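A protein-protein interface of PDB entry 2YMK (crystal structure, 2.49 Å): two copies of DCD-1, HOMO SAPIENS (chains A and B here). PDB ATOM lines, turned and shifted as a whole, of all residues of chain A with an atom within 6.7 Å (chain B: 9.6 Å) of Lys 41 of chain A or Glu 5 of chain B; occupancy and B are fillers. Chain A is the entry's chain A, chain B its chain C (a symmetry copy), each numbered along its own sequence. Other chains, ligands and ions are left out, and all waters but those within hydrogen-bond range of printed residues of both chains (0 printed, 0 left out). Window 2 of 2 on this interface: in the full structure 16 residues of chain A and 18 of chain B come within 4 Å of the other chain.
OG of Ser 2 of chain B is in hydrogen-bond range of N of Glu 5 of chain B, at 3.3 Å.
No position is printed for both chains.
Val 40 of chain A touches just one residue of chain B: Leu 8. Lys 41 of chain A touches just these residues of chain B: Glu 5 (3.2 Å) and Lys 12 (3.6 Å). No residue of chain B comes within 4 Å of Asp 42 of chain A. Printed residues of chain B within 4 Å of Leu 44 of chain A: Leu 4 and Leu 8. Glu 5 of chain B touches one residue of chain A. Of the printed residues of chain A, Leu 8 of chain B touches Val 37, Val 40 and Leu 44. Of the printed residues of chain A, Lys 12 of chain B touches Lys 34, Val 37 and Lys 41. The nearest residue of chain B that does not touch Lys 41 of chain A is Leu 8 of chain B (4.1 Å).
Of the 12 printed residues of chain B, 5 touch a printed residue of chain A. Printed residues of chain B that touch a printed residue of chain A: Leu 4, Glu 5, Leu 8, Ala 11 and Lys 12. Hydrophobic or aromatic side chains of chain B that line the printed part of chain A: Leu 4, Leu 8 and Ala 11. Of the 12 printed residues of chain A, 5 touch a printed residue of chain B. Among the printed residues, no Asp or Glu carboxylate lies within 4 Å of a Lys or Arg side-chain nitrogen of the other chain.
CG of Lys 34 of chain A touches CG of Lys 12 of chain B, 3.8 Å away. O of Leu 8 of chain B touches CG1 of Val 37 of chain A, at 3.0 Å. Ala 11 of chain B touches Val 37 of chain A (CB to CG2, 3.96 Å). Lys 12 of chain B touches Val 37 of chain A. CD2 of Leu 8 of chain B touches CG1 of Val 40 of chain A, 3.4 Å away. CG of Lys 41 of chain A touches OE2 of Glu 5 of chain B, at 3.2 Å. Lys 12 of chain B touches Lys 41 of chain A. Leu 44 of chain A touches Leu 4 of chain B. CD1 of Leu 8 of chain B touches CD2 of Leu 44 of chain A, 3.9 Å away.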
ATOM      1  N   LYS A  34     -24.106 -12.983  37.260  1.00  0.00           N
ATOM      2  CA  LYS A  34     -25.361 -12.308  37.075  1.00  0.00           C
ATOM      3  C   LYS A  34     -25.223 -10.778  36.952  1.00  0.00           C
ATOM      4  O   LYS A  34     -25.781 -10.179  35.990  1.00  0.00           O
ATOM      5  CB  LYS A  34     -26.351 -12.742  38.151  1.00  0.00           C
ATOM      6  CG  LYS A  34     -27.270 -13.918  37.664  1.00  0.00           C
ATOM      7  CD  LYS A  34     -27.848 -14.665  38.832  1.00  0.00           C
ATOM      8  CE  LYS A  34     -28.451 -15.976  38.452  1.00  0.00           C
ATOM      9  NZ  LYS A  34     -28.502 -16.709  39.732  1.00  0.00           N
ATOM     10  N   ALA A  36     -22.651  -9.446  35.665  1.00  0.00           N
ATOM     11  CA  ALA A  36     -22.040  -9.210  34.351  1.00  0.00           C
ATOM     12  C   ALA A  36     -23.096  -9.085  33.335  1.00  0.00           C
ATOM     13  O   ALA A  36     -23.155  -8.132  32.586  1.00  0.00           O
ATOM     14  CB  ALA A  36     -21.129 -10.339  33.969  1.00  0.00           C
ATOM     15  N   VAL A  37     -23.958 -10.075  33.313  1.00  0.00           N
ATOM     16  CA  VAL A  37     -25.111 -10.053  32.454  1.00  0.00           C
ATOM     17  C   VAL A  37     -25.953  -8.844  32.694  1.00  0.00           C
ATOM     18  O   VAL A  37     -26.359  -8.220  31.778  1.00  0.00           O
ATOM     19  CB  VAL A  37     -25.954 -11.260  32.673  1.00  0.00           C
ATOM     20  CG1 VAL A  37     -27.106 -11.179  31.747  1.00  0.00           C
ATOM     21  CG2 VAL A  37     -25.142 -12.526  32.356  1.00  0.00           C
ATOM     22  N   HIS A  38     -26.227  -8.495  33.936  1.00  0.00           N
ATOM     23  CA  HIS A  38     -26.951  -7.271  34.154  1.00  0.00           C
ATOM     24  C   HIS A  38     -26.221  -6.071  33.509  1.00  0.00           C
ATOM     25  O   HIS A  38     -26.794  -5.379  32.665  1.00  0.00           O
ATOM     26  CB  HIS A  38     -27.260  -7.033  35.631  1.00  0.00           C
ATOM     27  CG  HIS A  38     -28.048  -5.776  35.874  1.00  0.00           C
ATOM     28  ND1 HIS A  38     -29.418  -5.707  35.731  1.00  0.00           N
ATOM     29  CD2 HIS A  38     -27.651  -4.529  36.214  1.00  0.00           C
ATOM     30  CE1 HIS A  38     -29.831  -4.477  35.972  1.00  0.00           C
ATOM     31  NE2 HIS A  38     -28.777  -3.738  36.259  1.00  0.00           N
ATOM     32  N   ASP A  39     -24.954  -5.847  33.888  1.00  0.00           N
ATOM     33  CA  ASP A  39     -24.151  -4.753  33.406  1.00  0.00           C
ATOM     34  C   ASP A  39     -23.939  -4.709  31.890  1.00  0.00           C
ATOM     35  O   ASP A  39     -23.766  -3.611  31.325  1.00  0.00           O
ATOM     36  CB  ASP A  39     -22.827  -4.802  34.099  1.00  0.00           C
ATOM     37  CG  ASP A  39     -22.887  -4.345  35.564  1.00  0.00           C
ATOM     38  OD1 ASP A  39     -23.914  -3.824  36.044  1.00  0.00           O
ATOM     39  OD2 ASP A  39     -21.853  -4.500  36.255  1.00  0.00           O
ATOM     40  N   VAL A  40     -23.927  -5.875  31.228  1.00  0.00           N
ATOM     41  CA  VAL A  40     -24.035  -5.978  29.765  1.00  0.00           C
ATOM     42  C   VAL A  40     -25.423  -5.582  29.207  1.00  0.00           C
ATOM     43  O   VAL A  40     -25.504  -4.910  28.206  1.00  0.00           O
ATOM     44  CB  VAL A  40     -23.776  -7.394  29.280  1.00  0.00           C
ATOM     45  CG1 VAL A  40     -24.322  -7.539  27.900  1.00  0.00           C
ATOM     46  CG2 VAL A  40     -22.334  -7.718  29.266  1.00  0.00           C
ATOM     47  N   LYS A  41     -26.513  -6.025  29.820  1.00  0.00           N
ATOM     48  CA  LYS A  41     -27.843  -5.430  29.539  1.00  0.00           C
ATOM     49  C   LYS A  41     -27.725  -3.913  29.535  1.00  0.00           C
ATOM     50  O   LYS A  41     -27.991  -3.294  28.525  1.00  0.00           O
ATOM     51  CB  LYS A  41     -28.939  -5.809  30.587  1.00  0.00           C
ATOM     52  CG  LYS A  41     -29.648  -7.209  30.497  1.00  0.00           C
ATOM     53  CD  LYS A  41     -30.330  -7.583  31.859  1.00  0.00           C
ATOM     54  CE  LYS A  41     -30.237  -9.057  32.189  1.00  0.00           C
ATOM     55  NZ  LYS A  41     -30.268  -9.281  33.670  1.00  0.00           N
ATOM     56  N   ASP A  42     -27.354  -3.304  30.665  1.00  0.00           N
ATOM     57  CA  ASP A  42     -27.342  -1.849  30.784  1.00  0.00           C
ATOM     58  C   ASP A  42     -26.602  -1.169  29.671  1.00  0.00           C
ATOM     59  O   ASP A  42     -26.894  -0.040  29.354  1.00  0.00           O
ATOM     60  CB  ASP A  42     -26.677  -1.417  32.066  1.00  0.00           C
ATOM     61  CG  ASP A  42     -27.499  -1.706  33.273  1.00  0.00           C
ATOM     62  OD1 ASP A  42     -28.640  -2.199  33.139  1.00  0.00           O
ATOM     63  OD2 ASP A  42     -27.003  -1.435  34.386  1.00  0.00           O
ATOM     64  N   VAL A  43     -25.617  -1.834  29.092  1.00  0.00           N
ATOM     65  CA  VAL A  43     -24.782  -1.165  28.112  1.00  0.00           C
ATOM     66  C   VAL A  43     -25.369  -1.360  26.724  1.00  0.00           C
ATOM     67  O   VAL A  43     -25.516  -0.404  25.981  1.00  0.00           O
ATOM     68  CB  VAL A  43     -23.278  -1.518  28.224  1.00  0.00           C
ATOM     69  CG1 VAL A  43     -22.492  -0.602  27.359  1.00  0.00           C
ATOM     70  CG2 VAL A  43     -22.789  -1.363  29.647  1.00  0.00           C
ATOM     71  N   LEU A  44     -25.750  -2.577  26.380  1.00  0.00           N
ATOM     72  CA  LEU A  44     -26.494  -2.817  25.149  1.00  0.00           C
ATOM     73  C   LEU A  44     -27.853  -2.085  25.167  1.00  0.00           C
ATOM     74  O   LEU A  44     -28.661  -2.172  24.232  1.00  0.00           O
ATOM     75  CB  LEU A  44     -26.728  -4.323  25.001  1.00  0.00           C
ATOM     76  CG  LEU A  44     -25.797  -5.349  24.312  1.00  0.00           C
ATOM     77  CD1 LEU A  44     -24.338  -5.235  24.708  1.00  0.00           C
ATOM     78  CD2 LEU A  44     -26.307  -6.765  24.573  1.00  0.00           C
ATOM     79  N   ASP A  45     -28.084  -1.348  26.246  1.00  0.00           N
ATOM     80  CA  ASP A  45     -29.318  -0.582  26.459  1.00  0.00           C
ATOM     81  C   ASP A  45     -29.250   0.940  26.144  1.00  0.00           C
ATOM     82  O   ASP A  45     -30.209   1.519  25.647  1.00  0.00           O
ATOM     83  CB  ASP A  45     -29.709  -0.756  27.907  1.00  0.00           C
ATOM     84  CG  ASP A  45     -31.122  -1.130  28.075  1.00  0.00           C
ATOM     85  OD1 ASP A  45     -31.964  -0.228  27.921  1.00  0.00           O
ATOM     86  OD2 ASP A  45     -31.381  -2.313  28.389  1.00  0.00           O
ATOM     87  N   SER A  46     -28.131   1.589  26.461  1.00  0.00           N
ATOM     88  CA  SER A  46     -27.874   2.975  26.041  1.00  0.00           C
ATOM     89  C   SER A  46     -27.705   3.043  24.515  1.00  0.00           C
ATOM     90  O   SER A  46     -27.366   4.093  23.929  1.00  0.00           O
ATOM     91  CB  SER A  46     -26.648   3.539  26.774  1.00  0.00           C
ATOM     92  OG  SER A  46     -25.811   2.501  27.267  1.00  0.00           O
ATOM     93  N   SER B   2     -34.983  -9.852  20.790  1.00  0.00           N
ATOM     94  CA  SER B   2     -33.654  -9.777  20.095  1.00  0.00           C
ATOM     95  C   SER B   2     -32.945 -10.982  20.604  1.00  0.00           C
ATOM     96  O   SER B   2     -33.126 -11.323  21.764  1.00  0.00           O
ATOM     97  CB  SER B   2     -32.844  -8.527  20.495  1.00  0.00           C
ATOM     98  OG  SER B   2     -32.809  -8.357  21.911  1.00  0.00           O
ATOM     99  N   LEU B   3     -32.154 -11.616  19.741  1.00  0.00           N
ATOM    100  CA  LEU B   3     -31.273 -12.726  20.098  1.00  0.00           C
ATOM    101  C   LEU B   3     -30.438 -12.356  21.306  1.00  0.00           C
ATOM    102  O   LEU B   3     -30.183 -13.196  22.155  1.00  0.00           O
ATOM    103  CB  LEU B   3     -30.353 -13.026  18.915  1.00  0.00           C
ATOM    104  CG  LEU B   3     -31.126 -13.197  17.603  1.00  0.00           C
ATOM    105  CD1 LEU B   3     -30.352 -12.730  16.350  1.00  0.00           C
ATOM    106  CD2 LEU B   3     -31.620 -14.648  17.502  1.00  0.00           C
ATOM    107  N   LEU B   4     -30.048 -11.080  21.367  1.00  0.00           N
ATOM    108  CA  LEU B   4     -29.259 -10.507  22.456  1.00  0.00           C
ATOM    109  C   LEU B   4     -29.831 -10.649  23.849  1.00  0.00           C
ATOM    110  O   LEU B   4     -29.199 -11.275  24.670  1.00  0.00           O
ATOM    111  CB  LEU B   4     -28.918  -9.049  22.186  1.00  0.00           C
ATOM    112  CG  LEU B   4     -27.606  -8.950  21.435  1.00  0.00           C
ATOM    113  CD1 LEU B   4     -27.307  -7.508  21.032  1.00  0.00           C
ATOM    114  CD2 LEU B   4     -26.470  -9.601  22.258  1.00  0.00           C
ATOM    115  N   GLU B   5     -31.004 -10.083  24.130  1.00  0.00           N
ATOM    116  CA  GLU B   5     -31.562 -10.195  25.478  1.00  0.00           C
ATOM    117  C   GLU B   5     -31.786 -11.630  25.807  1.00  0.00           C
ATOM    118  O   GLU B   5     -31.703 -12.022  26.947  1.00  0.00           O
ATOM    119  CB  GLU B   5     -32.860  -9.416  25.667  1.00  0.00           C
ATOM    120  CG  GLU B   5     -32.710  -8.115  26.507  1.00  0.00           C
ATOM    121  CD  GLU B   5     -32.714  -8.326  28.031  1.00  0.00           C
ATOM    122  OE1 GLU B   5     -33.041  -9.437  28.505  1.00  0.00           O
ATOM    123  OE2 GLU B   5     -32.394  -7.363  28.769  1.00  0.00           O
ATOM    124  N   LYS B   6     -32.045 -12.424  24.792  1.00  0.00           N
ATOM    125  CA  LYS B   6     -32.328 -13.794  25.027  1.00  0.00           C
ATOM    126  C   LYS B   6     -31.028 -14.553  25.069  1.00  0.00           C
ATOM    127  O   LYS B   6     -30.939 -15.594  25.694  1.00  0.00           O
ATOM    128  CB  LYS B   6     -33.336 -14.317  24.008  1.00  0.00           C
ATOM    129  CG  LYS B   6     -34.825 -13.980  24.360  1.00  0.00           C
ATOM    130  CD  LYS B   6     -35.145 -14.204  25.852  1.00  0.00           C
ATOM    131  CE  LYS B   6     -36.564 -14.658  26.072  1.00  0.00           C
ATOM    132  NZ  LYS B   6     -36.612 -15.607  27.224  1.00  0.00           N
ATOM    133  N   GLY B   7     -29.993 -14.021  24.441  1.00  0.00           N
ATOM    134  CA  GLY B   7     -28.625 -14.463  24.744  1.00  0.00           C
ATOM    135  C   GLY B   7     -28.358 -14.276  26.223  1.00  0.00           C
ATOM    136  O   GLY B   7     -28.219 -15.230  26.925  1.00  0.00           O
ATOM    137  N   LEU B   8     -28.358 -13.043  26.703  1.00  0.00           N
ATOM    138  CA  LEU B   8     -27.949 -12.714  28.071  1.00  0.00           C
ATOM    139  C   LEU B   8     -28.680 -13.424  29.161  1.00  0.00           C
ATOM    140  O   LEU B   8     -28.108 -13.602  30.236  1.00  0.00           O
ATOM    141  CB  LEU B   8     -28.118 -11.221  28.340  1.00  0.00           C
ATOM    142  CG  LEU B   8     -27.565 -10.390  27.208  1.00  0.00           C
ATOM    143  CD1 LEU B   8     -28.243  -9.024  27.143  1.00  0.00           C
ATOM    144  CD2 LEU B   8     -26.052 -10.359  27.334  1.00  0.00           C
ATOM    145  N   ASP B   9     -29.952 -13.756  28.890  1.00  0.00           N
ATOM    146  CA  ASP B   9     -30.868 -14.454  29.813  1.00  0.00           C
ATOM    147  C   ASP B   9     -30.454 -15.882  29.830  1.00  0.00           C
ATOM    148  O   ASP B   9     -30.552 -16.562  30.825  1.00  0.00           O
ATOM    149  CB  ASP B   9     -32.322 -14.414  29.332  1.00  0.00           C
ATOM    150  CG  ASP B   9     -33.014 -13.063  29.583  1.00  0.00           C
ATOM    151  OD1 ASP B   9     -32.410 -12.185  30.277  1.00  0.00           O
ATOM    152  OD2 ASP B   9     -34.178 -12.891  29.100  1.00  0.00           O
ATOM    153  N   GLY B  10     -29.980 -16.355  28.706  1.00  0.00           N
ATOM    154  CA  GLY B  10     -29.425 -17.701  28.650  1.00  0.00           C
ATOM    155  C   GLY B  10     -28.078 -17.855  29.335  1.00  0.00           C
ATOM    156  O   GLY B  10     -27.742 -18.941  29.811  1.00  0.00           O
ATOM    157  N   ALA B  11     -27.300 -16.787  29.377  1.00  0.00           N
ATOM    158  CA  ALA B  11     -26.117 -16.783  30.172  1.00  0.00           C
ATOM    159  C   ALA B  11     -26.630 -16.748  31.621  1.00  0.00           C
ATOM    160  O   ALA B  11     -26.370 -17.660  32.400  1.00  0.00           O
ATOM    161  CB  ALA B  11     -25.284 -15.573  29.824  1.00  0.00           C
ATOM    162  N   LYS B  12     -27.389 -15.714  31.975  1.00  0.00           N
ATOM    163  CA  LYS B  12     -28.014 -15.611  33.305  1.00  0.00           C
ATOM    164  C   LYS B  12     -28.596 -16.962  33.737  1.00  0.00           C
ATOM    165  O   LYS B  12     -28.240 -17.456  34.803  1.00  0.00           O
ATOM    166  CB  LYS B  12     -29.087 -14.531  33.309  1.00  0.00           C
ATOM    167  CG  LYS B  12     -29.605 -14.094  34.636  1.00  0.00           C
ATOM    168  CD  LYS B  12     -30.900 -13.278  34.438  1.00  0.00           C
ATOM    169  CE  LYS B  12     -31.612 -12.864  35.751  1.00  0.00           C
ATOM    170  NZ  LYS B  12     -32.351 -11.576  35.585  1.00  0.00           N
ATOM    171  N   LYS B  13     -29.453 -17.590  32.916  1.00  0.00           N
ATOM    172  CA  LYS B  13     -29.991 -18.876  33.296  1.00  0.00           C
ATOM    173  C   LYS B  13     -28.860 -19.827  33.580  1.00  0.00           C
ATOM    174  O   LYS B  13     -28.866 -20.418  34.636  1.00  0.00           O
ATOM    175  CB  LYS B  13     -30.999 -19.402  32.299  1.00  0.00           C
ATOM    176  CG  LYS B  13     -32.367 -18.635  32.393  1.00  0.00           C
ATOM    177  CD  LYS B  13     -33.475 -19.174  31.426  1.00  0.00           C
ATOM    178  CE  LYS B  13     -34.920 -18.650  31.772  1.00  0.00           C
ATOM    179  NZ  LYS B  13     -36.105 -19.396  31.128  1.00  0.00           N
